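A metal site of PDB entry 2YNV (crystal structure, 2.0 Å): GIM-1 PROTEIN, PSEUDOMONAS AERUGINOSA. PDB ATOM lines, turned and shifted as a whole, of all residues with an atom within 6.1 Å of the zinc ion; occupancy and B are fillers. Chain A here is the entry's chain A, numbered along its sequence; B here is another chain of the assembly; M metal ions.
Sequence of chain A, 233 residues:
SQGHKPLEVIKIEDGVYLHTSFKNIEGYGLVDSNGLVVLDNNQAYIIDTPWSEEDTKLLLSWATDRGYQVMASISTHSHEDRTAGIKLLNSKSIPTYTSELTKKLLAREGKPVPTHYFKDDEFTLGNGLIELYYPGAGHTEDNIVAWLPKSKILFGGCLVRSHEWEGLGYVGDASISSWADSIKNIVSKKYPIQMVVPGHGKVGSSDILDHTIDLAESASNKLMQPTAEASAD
A ring nitrogen (ND1) of His 139 sits at hydrogen-bond distance from the backbone carbonyl oxygen of Tyr 170 (3.4 Å).
The guanidinium group (NE) of Arg 82 lies within salt-bridge range of OD1 of OCS 158, 3.0 Å away.
Merely in contact with the zinc ion: OCS 158.
Of the 10 residues printed, 4 come within 4 Å of the zinc ion.
The nearest printed residue that does not touch the zinc ion is Asp 81 (4.1 Å).
ND1 of His 79 is bound to the zinc ion, at 2.0 Å.
The zinc ion is bound by a ring nitrogen (NE2) of His 139.
NE2 of His 77 is bound to the zinc ion, 2.3 Å away.
The zinc ion has three donor atoms within binding distance.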
ATOM      1  N   HIS A  77     -15.402   1.734  24.736  1.00  0.00           N
ATOM      2  CA  HIS A  77     -16.560   1.570  23.955  1.00  0.00           C
ATOM      3  C   HIS A  77     -16.139   1.494  22.520  1.00  0.00           C
ATOM      4  O   HIS A  77     -14.953   1.340  22.204  1.00  0.00           O
ATOM      5  CB  HIS A  77     -17.602   2.665  24.119  1.00  0.00           C
ATOM      6  CG  HIS A  77     -17.098   4.031  23.820  1.00  0.00           C
ATOM      7  ND1 HIS A  77     -16.299   4.730  24.685  1.00  0.00           N
ATOM      8  CD2 HIS A  77     -17.316   4.838  22.740  1.00  0.00           C
ATOM      9  CE1 HIS A  77     -16.026   5.917  24.158  1.00  0.00           C
ATOM     10  NE2 HIS A  77     -16.608   5.981  22.973  1.00  0.00           N
ATOM     11  N   HIS A  79     -16.452   3.235  19.701  1.00  0.00           N
ATOM     12  CA  HIS A  79     -15.999   4.355  18.876  1.00  0.00           C
ATOM     13  C   HIS A  79     -14.495   4.463  18.627  1.00  0.00           C
ATOM     14  O   HIS A  79     -13.677   4.010  19.436  1.00  0.00           O
ATOM     15  CB  HIS A  79     -16.305   5.652  19.596  1.00  0.00           C
ATOM     16  CG  HIS A  79     -17.749   6.003  19.634  1.00  0.00           C
ATOM     17  ND1 HIS A  79     -18.251   6.977  20.487  1.00  0.00           N
ATOM     18  CD2 HIS A  79     -18.815   5.522  18.960  1.00  0.00           C
ATOM     19  CE1 HIS A  79     -19.560   7.047  20.351  1.00  0.00           C
ATOM     20  NE2 HIS A  79     -19.918   6.191  19.406  1.00  0.00           N
ATOM     21  N   ASP A  81     -12.021   6.782  18.841  1.00  0.00           N
ATOM     22  CA  ASP A  81     -11.019   7.273  19.805  1.00  0.00           C
ATOM     23  C   ASP A  81     -10.634   6.226  20.862  1.00  0.00           C
ATOM     24  O   ASP A  81      -9.766   6.472  21.719  1.00  0.00           O
ATOM     25  CB  ASP A  81     -11.430   8.584  20.512  1.00  0.00           C
ATOM     26  CG  ASP A  81     -12.788   8.501  21.207  1.00  0.00           C
ATOM     27  OD1 ASP A  81     -13.698   7.817  20.692  1.00  0.00           O
ATOM     28  OD2 ASP A  81     -12.950   9.167  22.255  1.00  0.00           O
ATOM     29  N   ARG A  82     -11.291   5.070  20.809  1.00  0.00           N
ATOM     30  CA  ARG A  82     -11.094   4.020  21.792  1.00  0.00           C
ATOM     31  C   ARG A  82     -10.551   2.753  21.113  1.00  0.00           C
ATOM     32  O   ARG A  82      -9.900   1.936  21.784  1.00  0.00           O
ATOM     33  CB  ARG A  82     -12.415   3.671  22.499  1.00  0.00           C
ATOM     34  CG  ARG A  82     -13.202   4.884  23.038  1.00  0.00           C
ATOM     35  CD  ARG A  82     -12.597   5.542  24.283  1.00  0.00           C
ATOM     36  NE  ARG A  82     -12.117   6.909  24.019  1.00  0.00           N
ATOM     37  CZ  ARG A  82     -11.123   7.539  24.673  1.00  0.00           C
ATOM     38  NH1 ARG A  82     -10.439   6.942  25.649  1.00  0.00           N
ATOM     39  NH2 ARG A  82     -10.791   8.766  24.338  1.00  0.00           N
ATOM     40  N   HIS A 139     -22.730   8.061  27.553  1.00  0.00           N
ATOM     41  CA  HIS A 139     -22.207   8.739  26.398  1.00  0.00           C
ATOM     42  C   HIS A 139     -22.460   7.746  25.269  1.00  0.00           C
ATOM     43  O   HIS A 139     -22.819   8.131  24.145  1.00  0.00           O
ATOM     44  CB  HIS A 139     -20.711   9.057  26.604  1.00  0.00           C
ATOM     45  CG  HIS A 139     -19.924   9.127  25.346  1.00  0.00           C
ATOM     46  ND1 HIS A 139     -19.974  10.206  24.505  1.00  0.00           N
ATOM     47  CD2 HIS A 139     -19.092   8.238  24.764  1.00  0.00           C
ATOM     48  CE1 HIS A 139     -19.201   9.987  23.457  1.00  0.00           C
ATOM     49  NE2 HIS A 139     -18.618   8.814  23.609  1.00  0.00           N
ATOM     50  N   THR A 140     -22.315   6.451  25.595  1.00  0.00           N
ATOM     51  CA  THR A 140     -22.820   5.418  24.662  1.00  0.00           C
ATOM     52  C   THR A 140     -23.604   4.354  25.354  1.00  0.00           C
ATOM     53  O   THR A 140     -23.673   4.340  26.588  1.00  0.00           O
ATOM     54  CB  THR A 140     -21.695   4.751  23.778  1.00  0.00           C
ATOM     55  OG1 THR A 140     -20.771   4.046  24.603  1.00  0.00           O
ATOM     56  CG2 THR A 140     -20.936   5.773  22.990  1.00  0.00           C
ATOM     57  N   OCS A 158     -15.256   8.345  28.198  1.00  0.00           N
ATOM     58  CA  OCS A 158     -16.163   9.403  27.772  1.00  0.00           C
ATOM     59  CB  OCS A 158     -16.456   9.368  26.295  1.00  0.00           C
ATOM     60  SG  OCS A 158     -15.027   9.883  25.309  1.00  0.00           S
ATOM     61  C   OCS A 158     -17.453   9.411  28.529  1.00  0.00           C
ATOM     62  O   OCS A 158     -18.291  10.277  28.289  1.00  0.00           O
ATOM     63  OD1 OCS A 158     -14.177   8.733  25.113  1.00  0.00           O
ATOM     64  OD2 OCS A 158     -15.509  10.367  24.024  1.00  0.00           O
ATOM     65  OD3 OCS A 158     -14.368  10.906  26.004  1.00  0.00           O
ATOM     66  N   TYR A 170     -20.321  14.685  22.113  1.00  0.00           N
ATOM     67  CA  TYR A 170     -21.186  14.044  21.134  1.00  0.00           C
ATOM     68  C   TYR A 170     -22.242  13.158  21.780  1.00  0.00           C
ATOM     69  O   TYR A 170     -21.888  12.158  22.442  1.00  0.00           O
ATOM     70  CB  TYR A 170     -20.366  13.206  20.159  1.00  0.00           C
ATOM     71  CG  TYR A 170     -21.258  12.500  19.183  1.00  0.00           C
ATOM     72  CD1 TYR A 170     -21.677  13.123  18.025  1.00  0.00           C
ATOM     73  CD2 TYR A 170     -21.726  11.221  19.432  1.00  0.00           C
ATOM     74  CE1 TYR A 170     -22.522  12.504  17.132  1.00  0.00           C
ATOM     75  CE2 TYR A 170     -22.566  10.577  18.549  1.00  0.00           C
ATOM     76  CZ  TYR A 170     -22.960  11.227  17.392  1.00  0.00           C
ATOM     77  OH  TYR A 170     -23.813  10.598  16.494  1.00  0.00           O
ATOM     78  N   GLU B  26     -16.274  10.681  16.029  1.00  0.00           N
ATOM     79  CA  GLU B  26     -15.186  10.015  16.735  1.00  0.00           C
ATOM     80  C   GLU B  26     -14.878  10.749  18.021  1.00  0.00           C
ATOM     81  O   GLU B  26     -13.777  11.253  18.167  1.00  0.00           O
ATOM     82  CB  GLU B  26     -13.898  10.032  15.924  1.00  0.00           C
ATOM     83  CG  GLU B  26     -13.969   9.414  14.564  1.00  0.00           C
ATOM     84  CD  GLU B  26     -12.651   9.547  13.837  1.00  0.00           C
ATOM     85  OE1 GLU B  26     -11.700   8.784  14.185  1.00  0.00           O
ATOM     86  OE2 GLU B  26     -12.553  10.436  12.950  1.00  0.00           O
ATOM     87  N   GLY B  27     -15.840  10.852  18.923  1.00  0.00           N
ATOM     88  CA  GLY B  27     -15.532  11.390  20.242  1.00  0.00           C
ATOM     89  C   GLY B  27     -15.200  12.869  20.271  1.00  0.00           C
ATOM     90  O   GLY B  27     -14.545  13.361  21.189  1.00  0.00           O
HETATM   91 ZN    ZN M   1     -17.527   7.907  22.092  1.00  0.00          ZN
